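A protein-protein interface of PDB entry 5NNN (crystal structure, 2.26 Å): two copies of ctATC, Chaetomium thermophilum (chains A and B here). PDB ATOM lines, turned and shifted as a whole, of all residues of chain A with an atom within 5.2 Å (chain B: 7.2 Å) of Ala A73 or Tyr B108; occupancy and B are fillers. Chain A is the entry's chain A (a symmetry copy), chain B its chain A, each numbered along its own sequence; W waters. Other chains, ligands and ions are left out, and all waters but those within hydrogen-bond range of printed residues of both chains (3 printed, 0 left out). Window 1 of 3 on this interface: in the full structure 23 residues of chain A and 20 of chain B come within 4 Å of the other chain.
Of chain B, only Ile B83 (3.4 Å) and Tyr B108 (3.7 Å) come within 4 Å of Ala A73.
Of the printed residues of chain A, Tyr B108 touches Arg A66, Ser A70, Ala A73, Arg A77 and Met A299.
Of the printed residues of chain A, Ile B85 touches Ala A69 (3.8 Å).
Of the printed residues of chain A, Leu B105 touches Thr A65 (3.8 Å) and Ala A69 (3.9 Å).
Printed residues of chain A within 4 Å of Val B55: Arg A77 (3.5 Å).
Of the printed residues of chain A, Thr B82 touches Gln A76.
The nearest printed residue of chain A that does not touch Tyr B108 is Ala A69 (4.01 Å).
The nearest printed residue of chain A that does not touch Asp B110 is Arg A300 (6.8 Å).
Hydrophobic or aromatic side chains of chain B that line the printed part of chain A: Val B55, Ile B83, Ile B85, Leu B105 and Tyr B108.
Hydrophobic or aromatic side chains of chain A that line the printed part of chain B: Ala A69, Ala A73, Met A299 and Leu A303.
Among the printed residues, Asp or Glu carboxylates within 4 Å of a Lys or Arg side-chain nitrogen of the other chain: Arg A77 with Asp B110 (3.4 Å).
No position is printed for both chains.
Of the 20 pairs that touch across the chains among the printed residues, none has its exchanged pair printed and touching as well.
Water W3 lies within hydrogen-bond range of the side-chain amide oxygen of Gln A76 and the backbone NH of Thr B82.
Water W1 lies within hydrogen-bond range of OD2 of Asp A72 (2.6 Å) and O of Thr B82 (3.3 Å).
Water W2 lies within hydrogen-bond range of O of Met A299 (2.9 Å), OH of Tyr B108 (2.9 Å), OG of Ser A70 (3.0 Å) and NH1 of Arg A306 (3.3 Å).
NE2 of Gln A76 sits at hydrogen-bond distance from O of Thr B82, at 3.0 Å.
NH2 of Arg A66 lies within hydrogen-bond range of OG1 of Thr B104 (3.2 Å).
OG1 of Thr B104 lies close to SD of Met A299.
The backbone carbonyl oxygen of Arg A66 lies within hydrogen-bond range of the side-chain hydroxyl of Tyr B108, at 3.1 Å.
The guanidinium group (NH2) of Arg A77 lies within hydrogen-bond range of the backbone carbonyl oxygen (O) of Tyr B108, 3.0 Å away.
NH2 of Arg A77 lies within salt-bridge range of OD1 of Asp B110, at 3.4 Å.
The backbone carbonyl oxygen (O) of Val B55 sits at hydrogen-bond distance from the backbone NH (N) of Asp B110 (2.7 Å).
O of Leu B56 lies within hydrogen-bond range of N of Ile B83 (2.9 Å).
The side-chain amide nitrogen of Asn B107 lies within hydrogen-bond range of the backbone carbonyl oxygen of Thr B104.
OG of Ser B109 lies within hydrogen-bond range of O of Leu B105, at 3.1 Å.
The backbone carbonyl oxygen of Ala B111 is in hydrogen-bond range of the side-chain hydroxyl of Ser B109, 3.5 Å away.
The side-chain hydroxyl (OG) of Ser A70 sits at hydrogen-bond distance from the guanidinium group (NH1) of Arg A306.
Among the printed residues, pairs that only touch across the chains: Thr A65 with Leu B105, Ala A69 with Ile B85, Ala A69 with Leu B105, Ser A70 with Tyr B108, Asp A72 with Ile B83, Ala A73 with Ile B83, Ala A73 with Tyr B108, Gln A76 with Ile B83, Arg A77 with Val B55, Arg A77 with Ser B109, Met A299 with Asn B107, Met A299 with Tyr B108, Arg A300 with Asn B107 and Leu A303 with Asn B107.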
ATOM      1  N   THR A  65     -24.852   1.252  -0.730  1.00  0.00           N
ATOM      2  CA  THR A  65     -24.217   1.276   0.588  1.00  0.00           C
ATOM      3  C   THR A  65     -22.754   1.719   0.528  1.00  0.00           C
ATOM      4  O   THR A  65     -22.290   2.487   1.375  1.00  0.00           O
ATOM      5  CB  THR A  65     -24.318  -0.132   1.215  1.00  0.00           C
ATOM      6  OG1 THR A  65     -25.690  -0.483   1.448  1.00  0.00           O
ATOM      7  CG2 THR A  65     -23.572  -0.195   2.567  1.00  0.00           C
ATOM      8  N   ARG A  66     -21.987   1.194  -0.419  1.00  0.00           N
ATOM      9  CA  ARG A  66     -20.577   1.547  -0.471  1.00  0.00           C
ATOM     10  C   ARG A  66     -20.395   3.034  -0.679  1.00  0.00           C
ATOM     11  O   ARG A  66     -19.606   3.688   0.024  1.00  0.00           O
ATOM     12  CB  ARG A  66     -19.892   0.728  -1.558  1.00  0.00           C
ATOM     13  CG  ARG A  66     -19.285   1.446  -2.773  1.00  0.00           C
ATOM     14  CD  ARG A  66     -19.053   0.371  -3.872  1.00  0.00           C
ATOM     15  NE  ARG A  66     -18.795  -0.842  -3.115  1.00  0.00           N
ATOM     16  CZ  ARG A  66     -19.559  -1.923  -3.081  1.00  0.00           C
ATOM     17  NH1 ARG A  66     -20.632  -2.020  -3.863  1.00  0.00           N
ATOM     18  NH2 ARG A  66     -19.215  -2.922  -2.253  1.00  0.00           N
ATOM     19  N   THR A  67     -21.188   3.612  -1.567  1.00  0.00           N
ATOM     20  CA  THR A  67     -21.055   5.031  -1.852  1.00  0.00           C
ATOM     21  C   THR A  67     -21.718   5.892  -0.785  1.00  0.00           C
ATOM     22  O   THR A  67     -21.126   6.878  -0.308  1.00  0.00           O
ATOM     23  CB  THR A  67     -21.641   5.294  -3.232  1.00  0.00           C
ATOM     24  OG1 THR A  67     -20.988   4.464  -4.179  1.00  0.00           O
ATOM     25  CG2 THR A  67     -21.413   6.668  -3.626  1.00  0.00           C
ATOM     26  N   SER A  68     -22.936   5.550  -0.372  1.00  0.00           N
ATOM     27  CA  SER A  68     -23.626   6.421   0.581  1.00  0.00           C
ATOM     28  C   SER A  68     -22.928   6.406   1.930  1.00  0.00           C
ATOM     29  O   SER A  68     -22.747   7.460   2.550  1.00  0.00           O
ATOM     30  CB  SER A  68     -25.101   6.034   0.743  1.00  0.00           C
ATOM     31  OG  SER A  68     -25.243   4.792   1.375  1.00  0.00           O
ATOM     32  N   ALA A  69     -22.549   5.224   2.414  1.00  0.00           N
ATOM     33  CA  ALA A  69     -21.867   5.182   3.697  1.00  0.00           C
ATOM     34  C   ALA A  69     -20.459   5.787   3.601  1.00  0.00           C
ATOM     35  O   ALA A  69     -19.979   6.376   4.575  1.00  0.00           O
ATOM     36  CB  ALA A  69     -21.784   3.752   4.180  1.00  0.00           C
ATOM     37  N   SER A  70     -19.772   5.622   2.462  1.00  0.00           N
ATOM     38  CA  SER A  70     -18.489   6.320   2.280  1.00  0.00           C
ATOM     39  C   SER A  70     -18.629   7.828   2.449  1.00  0.00           C
ATOM     40  O   SER A  70     -17.827   8.467   3.149  1.00  0.00           O
ATOM     41  CB  SER A  70     -17.918   6.034   0.884  1.00  0.00           C
ATOM     42  OG  SER A  70     -16.691   6.719   0.723  1.00  0.00           O
ATOM     43  N   PHE A  71     -19.625   8.442   1.789  1.00  0.00           N
ATOM     44  CA  PHE A  71     -19.804   9.887   2.001  1.00  0.00           C
ATOM     45  C   PHE A  71     -20.266  10.229   3.408  1.00  0.00           C
ATOM     46  O   PHE A  71     -19.913  11.303   3.938  1.00  0.00           O
ATOM     47  CB  PHE A  71     -20.781  10.479   1.017  1.00  0.00           C
ATOM     48  CG  PHE A  71     -20.219  10.700  -0.370  1.00  0.00           C
ATOM     49  CD1 PHE A  71     -19.395  11.791  -0.644  1.00  0.00           C
ATOM     50  CD2 PHE A  71     -20.535   9.843  -1.395  1.00  0.00           C
ATOM     51  CE1 PHE A  71     -18.914  12.002  -1.939  1.00  0.00           C
ATOM     52  CE2 PHE A  71     -20.060  10.045  -2.720  1.00  0.00           C
ATOM     53  CZ  PHE A  71     -19.259  11.130  -2.976  1.00  0.00           C
ATOM     54  N   ASP A  72     -21.091   9.388   4.022  1.00  0.00           N
ATOM     55  CA  ASP A  72     -21.524   9.671   5.395  1.00  0.00           C
ATOM     56  C   ASP A  72     -20.303   9.714   6.295  1.00  0.00           C
ATOM     57  O   ASP A  72     -20.054  10.702   6.993  1.00  0.00           O
ATOM     58  CB  ASP A  72     -22.509   8.592   5.880  1.00  0.00           C
ATOM     59  CG  ASP A  72     -23.238   8.985   7.131  1.00  0.00           C
ATOM     60  OD1 ASP A  72     -22.872  10.036   7.685  1.00  0.00           O
ATOM     61  OD2 ASP A  72     -24.186   8.266   7.554  1.00  0.00           O
ATOM     62  N   ALA A  73     -19.475   8.675   6.199  1.00  0.00           N
ATOM     63  CA  ALA A  73     -18.299   8.552   7.054  1.00  0.00           C
ATOM     64  C   ALA A  73     -17.273   9.630   6.738  1.00  0.00           C
ATOM     65  O   ALA A  73     -16.689  10.203   7.654  1.00  0.00           O
ATOM     66  CB  ALA A  73     -17.677   7.169   6.900  1.00  0.00           C
ATOM     67  N   ALA A  74     -17.121  10.005   5.465  1.00  0.00           N
ATOM     68  CA  ALA A  74     -16.226  11.109   5.160  1.00  0.00           C
ATOM     69  C   ALA A  74     -16.712  12.393   5.806  1.00  0.00           C
ATOM     70  O   ALA A  74     -15.971  13.048   6.546  1.00  0.00           O
ATOM     71  CB  ALA A  74     -16.070  11.281   3.650  1.00  0.00           C
ATOM     72  N   MET A  75     -17.964  12.770   5.576  1.00  0.00           N
ATOM     73  CA  MET A  75     -18.411  14.011   6.196  1.00  0.00           C
ATOM     74  C   MET A  75     -18.188  13.977   7.701  1.00  0.00           C
ATOM     75  O   MET A  75     -17.651  14.936   8.288  1.00  0.00           O
ATOM     76  CB  MET A  75     -19.866  14.297   5.912  1.00  0.00           C
ATOM     77  CG  MET A  75     -20.238  15.639   6.463  1.00  0.00           C
ATOM     78  SD  MET A  75     -19.426  16.928   5.466  1.00  0.00           S
ATOM     79  CE  MET A  75     -20.356  18.330   6.046  1.00  0.00           C
ATOM     80  N   GLN A  76     -18.606  12.890   8.357  1.00  0.00           N
ATOM     81  CA  GLN A  76     -18.559  12.903   9.813  1.00  0.00           C
ATOM     82  C   GLN A  76     -17.113  12.924  10.315  1.00  0.00           C
ATOM     83  O   GLN A  76     -16.824  13.488  11.377  1.00  0.00           O
ATOM     84  CB  GLN A  76     -19.320  11.699  10.391  1.00  0.00           C
ATOM     85  CG  GLN A  76     -20.838  11.830  10.209  1.00  0.00           C
ATOM     86  CD  GLN A  76     -21.661  10.931  11.081  1.00  0.00           C
ATOM     87  OE1 GLN A  76     -21.765  11.146  12.297  1.00  0.00           O
ATOM     88  NE2 GLN A  76     -22.325   9.947  10.456  1.00  0.00           N
ATOM     89  N   ARG A  77     -16.204  12.299   9.588  1.00  0.00           N
ATOM     90  CA  ARG A  77     -14.823  12.303  10.014  1.00  0.00           C
ATOM     91  C   ARG A  77     -14.146  13.646   9.749  1.00  0.00           C
ATOM     92  O   ARG A  77     -13.105  13.912  10.343  1.00  0.00           O
ATOM     93  CB  ARG A  77     -14.073  11.173   9.337  1.00  0.00           C
ATOM     94  CG  ARG A  77     -14.217   9.813  10.035  1.00  0.00           C
ATOM     95  CD  ARG A  77     -13.312   8.807   9.370  1.00  0.00           C
ATOM     96  NE  ARG A  77     -13.524   7.400   9.764  1.00  0.00           N
ATOM     97  CZ  ARG A  77     -13.253   6.905  10.969  1.00  0.00           C
ATOM     98  NH1 ARG A  77     -12.799   7.684  11.929  1.00  0.00           N
ATOM     99  NH2 ARG A  77     -13.448   5.627  11.222  1.00  0.00           N
ATOM    100  N   LEU A  78     -14.724  14.497   8.891  1.00  0.00           N
ATOM    101  CA  LEU A  78     -14.344  15.895   8.777  1.00  0.00           C
ATOM    102  C   LEU A  78     -14.911  16.762   9.900  1.00  0.00           C
ATOM    103  O   LEU A  78     -14.603  17.974   9.976  1.00  0.00           O
ATOM    104  CB  LEU A  78     -14.790  16.457   7.426  1.00  0.00           C
ATOM    105  CG  LEU A  78     -14.047  15.917   6.188  1.00  0.00           C
ATOM    106  CD1 LEU A  78     -14.706  16.447   4.945  1.00  0.00           C
ATOM    107  CD2 LEU A  78     -12.573  16.301   6.162  1.00  0.00           C
ATOM    108  N   MET A 299     -11.688   1.018  -1.242  1.00  0.00           N
ATOM    109  CA  MET A 299     -12.710   1.784  -0.560  1.00  0.00           C
ATOM    110  C   MET A 299     -12.128   2.636   0.558  1.00  0.00           C
ATOM    111  O   MET A 299     -12.642   3.727   0.838  1.00  0.00           O
ATOM    112  CB  MET A 299     -13.800   0.823  -0.098  1.00  0.00           C
ATOM    113  CG  MET A 299     -14.774   0.442  -1.317  1.00  0.00           C
ATOM    114  SD  MET A 299     -15.736  -0.993  -1.144  1.00  0.00           S
ATOM    115  CE  MET A 299     -14.644  -2.138  -0.401  1.00  0.00           C
ATOM    116  N   ARG A 300     -11.060   2.191   1.209  1.00  0.00           N
ATOM    117  CA  ARG A 300     -10.421   3.088   2.172  1.00  0.00           C
ATOM    118  C   ARG A 300      -9.753   4.262   1.442  1.00  0.00           C
ATOM    119  O   ARG A 300      -9.864   5.432   1.876  1.00  0.00           O
ATOM    120  CB  ARG A 300      -9.432   2.304   3.066  1.00  0.00           C
ATOM    121  CG  ARG A 300      -9.036   3.109   4.345  1.00  0.00           C
ATOM    122  CD  ARG A 300      -7.923   2.478   5.122  1.00  0.00           C
ATOM    123  NE  ARG A 300      -8.317   1.227   5.754  1.00  0.00           N
ATOM    124  CZ  ARG A 300      -9.112   1.143   6.814  1.00  0.00           C
ATOM    125  NH1 ARG A 300      -9.635   2.240   7.374  1.00  0.00           N
ATOM    126  NH2 ARG A 300      -9.384  -0.050   7.313  1.00  0.00           N
ATOM    127  N   LEU A 303     -12.481   6.592   0.886  1.00  0.00           N
ATOM    128  CA  LEU A 303     -12.727   7.408   2.066  1.00  0.00           C
ATOM    129  C   LEU A 303     -11.858   8.666   2.050  1.00  0.00           C
ATOM    130  O   LEU A 303     -12.370   9.793   2.180  1.00  0.00           O
ATOM    131  CB  LEU A 303     -12.515   6.586   3.324  1.00  0.00           C
ATOM    132  CG  LEU A 303     -12.748   7.406   4.590  1.00  0.00           C
ATOM    133  CD1 LEU A 303     -14.233   7.695   4.810  1.00  0.00           C
ATOM    134  CD2 LEU A 303     -12.139   6.680   5.782  1.00  0.00           C
ATOM    135  N   ARG A 306     -12.809  11.209  -0.690  1.00  0.00           N
ATOM    136  CA  ARG A 306     -14.054  11.953  -0.509  1.00  0.00           C
ATOM    137  C   ARG A 306     -13.954  12.924   0.647  1.00  0.00           C
ATOM    138  O   ARG A 306     -14.590  13.982   0.600  1.00  0.00           O
ATOM    139  CB  ARG A 306     -15.259  11.006  -0.325  1.00  0.00           C
ATOM    140  CG  ARG A 306     -15.664  10.341  -1.631  1.00  0.00           C
ATOM    141  CD  ARG A 306     -16.547   9.124  -1.479  1.00  0.00           C
ATOM    142  NE  ARG A 306     -16.865   8.659  -2.822  1.00  0.00           N
ATOM    143  CZ  ARG A 306     -17.071   7.405  -3.186  1.00  0.00           C
ATOM    144  NH1 ARG A 306     -17.039   6.430  -2.290  1.00  0.00           N
ATOM    145  NH2 ARG A 306     -17.278   7.125  -4.473  1.00  0.00           N
ATOM    146  N   VAL B  55     -16.115   5.881  15.101  1.00  0.00           N
ATOM    147  CA  VAL B  55     -17.277   5.724  14.235  1.00  0.00           C
ATOM    148  C   VAL B  55     -17.788   4.292  14.370  1.00  0.00           C
ATOM    149  O   VAL B  55     -17.027   3.335  14.170  1.00  0.00           O
ATOM    150  CB  VAL B  55     -16.925   6.038  12.773  1.00  0.00           C
ATOM    151  CG1 VAL B  55     -18.162   5.850  11.868  1.00  0.00           C
ATOM    152  CG2 VAL B  55     -16.293   7.450  12.654  1.00  0.00           C
ATOM    153  N   LEU B  56     -19.063   4.149  14.718  1.00  0.00           N
ATOM    154  CA  LEU B  56     -19.742   2.865  14.771  1.00  0.00           C
ATOM    155  C   LEU B  56     -20.721   2.782  13.614  1.00  0.00           C
ATOM    156  O   LEU B  56     -21.515   3.709  13.387  1.00  0.00           O
ATOM    157  CB  LEU B  56     -20.513   2.667  16.077  1.00  0.00           C
ATOM    158  CG  LEU B  56     -21.363   1.370  16.169  1.00  0.00           C
ATOM    159  CD1 LEU B  56     -20.455   0.143  16.416  1.00  0.00           C
ATOM    160  CD2 LEU B  56     -22.347   1.413  17.295  1.00  0.00           C
ATOM    161  N   CYS B  57     -20.708   1.661  12.921  1.00  0.00           N
ATOM    162  CA  CYS B  57     -21.670   1.401  11.868  1.00  0.00           C
ATOM    163  C   CYS B  57     -22.615   0.288  12.306  1.00  0.00           C
ATOM    164  O   CYS B  57     -22.160  -0.769  12.744  1.00  0.00           O
ATOM    165  CB  CYS B  57     -20.935   1.019  10.601  1.00  0.00           C
ATOM    166  SG  CYS B  57     -21.881   0.030   9.556  1.00  0.00           S
ATOM    167  N   THR B  82     -22.134   7.675  14.442  1.00  0.00           N
ATOM    168  CA  THR B  82     -22.831   6.485  13.955  1.00  0.00           C
ATOM    169  C   THR B  82     -23.197   6.608  12.472  1.00  0.00           C
ATOM    170  O   THR B  82     -23.567   7.689  11.978  1.00  0.00           O
ATOM    171  CB  THR B  82     -24.129   6.250  14.738  1.00  0.00           C
ATOM    172  OG1 THR B  82     -24.989   7.386  14.526  1.00  0.00           O
ATOM    173  CG2 THR B  82     -23.844   6.045  16.232  1.00  0.00           C
ATOM    174  N   ILE B  83     -23.105   5.475  11.792  1.00  0.00           N
ATOM    175  CA  ILE B  83     -23.583   5.283  10.425  1.00  0.00           C
ATOM    176  C   ILE B  83     -24.566   4.108  10.422  1.00  0.00           C
ATOM    177  O   ILE B  83     -24.167   2.938  10.378  1.00  0.00           O
ATOM    178  CB  ILE B  83     -22.414   5.023   9.456  1.00  0.00           C
ATOM    179  CG1 ILE B  83     -21.446   6.206   9.506  1.00  0.00           C
ATOM    180  CG2 ILE B  83     -22.926   4.821   8.027  1.00  0.00           C
ATOM    181  CD1 ILE B  83     -20.199   5.938   8.747  1.00  0.00           C
ATOM    182  N   ILE B  85     -27.069   1.607   8.784  1.00  0.00           N
ATOM    183  CA  ILE B  85     -27.374   0.988   7.500  1.00  0.00           C
ATOM    184  C   ILE B  85     -28.597   0.061   7.671  1.00  0.00           C
ATOM    185  O   ILE B  85     -28.582  -0.899   8.488  1.00  0.00           O
ATOM    186  CB  ILE B  85     -26.175   0.169   6.972  1.00  0.00           C
ATOM    187  CG1 ILE B  85     -24.791   0.847   7.122  1.00  0.00           C
ATOM    188  CG2 ILE B  85     -26.470  -0.389   5.544  1.00  0.00           C
ATOM    189  CD1 ILE B  85     -24.393   1.771   6.129  1.00  0.00           C
ATOM    190  N   THR B 101     -19.940  -6.977   2.162  1.00  0.00           N
ATOM    191  CA  THR B 101     -20.464  -5.773   2.826  1.00  0.00           C
ATOM    192  C   THR B 101     -19.666  -5.448   4.087  1.00  0.00           C
ATOM    193  O   THR B 101     -19.323  -4.290   4.336  1.00  0.00           O
ATOM    194  CB  THR B 101     -21.957  -5.961   3.146  1.00  0.00           C
ATOM    195  OG1 THR B 101     -22.694  -6.117   1.912  1.00  0.00           O
ATOM    196  CG2 THR B 101     -22.495  -4.736   3.909  1.00  0.00           C
ATOM    197  N   LEU B 102     -19.341  -6.460   4.889  1.00  0.00           N
ATOM    198  CA  LEU B 102     -18.541  -6.224   6.088  1.00  0.00           C
ATOM    199  C   LEU B 102     -17.193  -5.614   5.736  1.00  0.00           C
ATOM    200  O   LEU B 102     -16.763  -4.614   6.334  1.00  0.00           O
ATOM    201  CB  LEU B 102     -18.348  -7.545   6.835  1.00  0.00           C
ATOM    202  CG  LEU B 102     -19.587  -8.054   7.554  1.00  0.00           C
ATOM    203  CD1 LEU B 102     -19.311  -9.422   8.071  1.00  0.00           C
ATOM    204  CD2 LEU B 102     -19.946  -7.079   8.679  1.00  0.00           C
ATOM    205  N   ARG B 103     -16.509  -6.189   4.758  1.00  0.00           N
ATOM    206  CA  ARG B 103     -15.210  -5.622   4.406  1.00  0.00           C
ATOM    207  C   ARG B 103     -15.363  -4.232   3.806  1.00  0.00           C
ATOM    208  O   ARG B 103     -14.555  -3.351   4.080  1.00  0.00           O
ATOM    209  CB  ARG B 103     -14.482  -6.606   3.495  1.00  0.00           C
ATOM    210  CG  ARG B 103     -13.840  -7.848   4.320  1.00  0.00           C
ATOM    211  CD  ARG B 103     -13.355  -8.948   3.393  1.00  0.00           C
ATOM    212  NE  ARG B 103     -14.425  -9.517   2.583  1.00  0.00           N
ATOM    213  CZ  ARG B 103     -14.274 -10.526   1.741  1.00  0.00           C
ATOM    214  NH1 ARG B 103     -13.084 -11.121   1.616  1.00  0.00           N
ATOM    215  NH2 ARG B 103     -15.322 -10.982   1.047  1.00  0.00           N
ATOM    216  N   THR B 104     -16.458  -3.968   3.080  1.00  0.00           N
ATOM    217  CA  THR B 104     -16.694  -2.604   2.612  1.00  0.00           C
ATOM    218  C   THR B 104     -16.749  -1.626   3.772  1.00  0.00           C
ATOM    219  O   THR B 104     -16.036  -0.606   3.782  1.00  0.00           O
ATOM    220  CB  THR B 104     -17.988  -2.553   1.831  1.00  0.00           C
ATOM    221  OG1 THR B 104     -17.825  -3.323   0.626  1.00  0.00           O
ATOM    222  CG2 THR B 104     -18.360  -1.084   1.542  1.00  0.00           C
ATOM    223  N   LEU B 105     -17.623  -1.914   4.745  1.00  0.00           N
ATOM    224  CA  LEU B 105     -17.941  -1.000   5.836  1.00  0.00           C
ATOM    225  C   LEU B 105     -16.833  -0.897   6.894  1.00  0.00           C
ATOM    226  O   LEU B 105     -16.687   0.146   7.566  1.00  0.00           O
ATOM    227  CB  LEU B 105     -19.245  -1.472   6.481  1.00  0.00           C
ATOM    228  CG  LEU B 105     -20.496  -1.328   5.589  1.00  0.00           C
ATOM    229  CD1 LEU B 105     -21.689  -1.782   6.402  1.00  0.00           C
ATOM    230  CD2 LEU B 105     -20.713   0.130   5.107  1.00  0.00           C
ATOM    231  N   ALA B 106     -16.055  -1.968   7.059  1.00  0.00           N
ATOM    232  CA  ALA B 106     -14.893  -1.917   7.933  1.00  0.00           C
ATOM    233  C   ALA B 106     -13.925  -0.800   7.552  1.00  0.00           C
ATOM    234  O   ALA B 106     -13.269  -0.244   8.428  1.00  0.00           O
ATOM    235  CB  ALA B 106     -14.205  -3.278   7.926  1.00  0.00           C
ATOM    236  N   ASN B 107     -13.849  -0.419   6.269  1.00  0.00           N
ATOM    237  CA  ASN B 107     -13.015   0.733   5.881  1.00  0.00           C
ATOM    238  C   ASN B 107     -13.555   2.089   6.324  1.00  0.00           C
ATOM    239  O   ASN B 107     -12.846   3.100   6.161  1.00  0.00           O
ATOM    240  CB  ASN B 107     -12.843   0.817   4.351  1.00  0.00           C
ATOM    241  CG  ASN B 107     -12.111  -0.366   3.796  1.00  0.00           C
ATOM    242  OD1 ASN B 107     -10.932  -0.556   4.075  1.00  0.00           O
ATOM    243  ND2 ASN B 107     -12.804  -1.180   3.024  1.00  0.00           N
ATOM    244  N   TYR B 108     -14.787   2.160   6.823  1.00  0.00           N
ATOM    245  CA  TYR B 108     -15.369   3.439   7.207  1.00  0.00           C
ATOM    246  C   TYR B 108     -15.494   3.613   8.701  1.00  0.00           C
ATOM    247  O   TYR B 108     -15.507   4.738   9.183  1.00  0.00           O
ATOM    248  CB  TYR B 108     -16.775   3.591   6.590  1.00  0.00           C
ATOM    249  CG  TYR B 108     -16.802   3.395   5.105  1.00  0.00           C
ATOM    250  CD1 TYR B 108     -15.690   3.715   4.317  1.00  0.00           C
ATOM    251  CD2 TYR B 108     -17.894   2.825   4.489  1.00  0.00           C
ATOM    252  CE1 TYR B 108     -15.695   3.493   2.983  1.00  0.00           C
ATOM    253  CE2 TYR B 108     -17.905   2.620   3.121  1.00  0.00           C
ATOM    254  CZ  TYR B 108     -16.818   2.989   2.373  1.00  0.00           C
ATOM    255  OH  TYR B 108     -16.810   2.739   1.014  1.00  0.00           O
ATOM    256  N   SER B 109     -15.627   2.528   9.433  1.00  0.00           N
ATOM    257  CA  SER B 109     -15.951   2.600  10.844  1.00  0.00           C
ATOM    258  C   SER B 109     -14.937   1.787  11.651  1.00  0.00           C
ATOM    259  O   SER B 109     -14.207   0.927  11.134  1.00  0.00           O
ATOM    260  CB  SER B 109     -17.365   2.065  11.081  1.00  0.00           C
ATOM    261  OG  SER B 109     -17.433   0.788  10.482  1.00  0.00           O
ATOM    262  N   ASP B 110     -14.935   2.049  12.941  1.00  0.00           N
ATOM    263  CA  ASP B 110     -14.079   1.337  13.874  1.00  0.00           C
ATOM    264  C   ASP B 110     -14.739   0.094  14.446  1.00  0.00           C
ATOM    265  O   ASP B 110     -14.059  -0.728  15.039  1.00  0.00           O
ATOM    266  CB  ASP B 110     -13.657   2.324  14.980  1.00  0.00           C
ATOM    267  CG  ASP B 110     -13.051   3.609  14.389  1.00  0.00           C
ATOM    268  OD1 ASP B 110     -12.150   3.503  13.515  1.00  0.00           O
ATOM    269  OD2 ASP B 110     -13.514   4.715  14.723  1.00  0.00           O
ATOM    270  N   ALA B 111     -16.025  -0.114  14.213  1.00  0.00           N
ATOM    271  CA  ALA B 111     -16.678  -1.352  14.616  1.00  0.00           C
ATOM    272  C   ALA B 111     -18.057  -1.403  13.969  1.00  0.00           C
ATOM    273  O   ALA B 111     -18.590  -0.378  13.549  1.00  0.00           O
ATOM    274  CB  ALA B 111     -16.808  -1.434  16.121  1.00  0.00           C
ATOM    275  N   VAL B 131     -12.501  -5.450  11.699  1.00  0.00           N
ATOM    276  CA  VAL B 131     -12.793  -4.584  12.844  1.00  0.00           C
ATOM    277  C   VAL B 131     -13.717  -5.362  13.764  1.00  0.00           C
ATOM    278  O   VAL B 131     -14.356  -6.332  13.331  1.00  0.00           O
ATOM    279  CB  VAL B 131     -13.441  -3.242  12.432  1.00  0.00           C
ATOM    280  CG1 VAL B 131     -12.534  -2.501  11.472  1.00  0.00           C
ATOM    281  CG2 VAL B 131     -14.880  -3.441  11.842  1.00  0.00           C
HETATM  282  O   HOH W   1     -25.615   8.810   9.706  1.00  0.00           O
HETATM  283  O   HOH W   2     -15.074   4.526  -0.429  1.00  0.00           O
HETATM  284  O   HOH W   3     -23.476  10.635  14.222  1.00  0.00           O
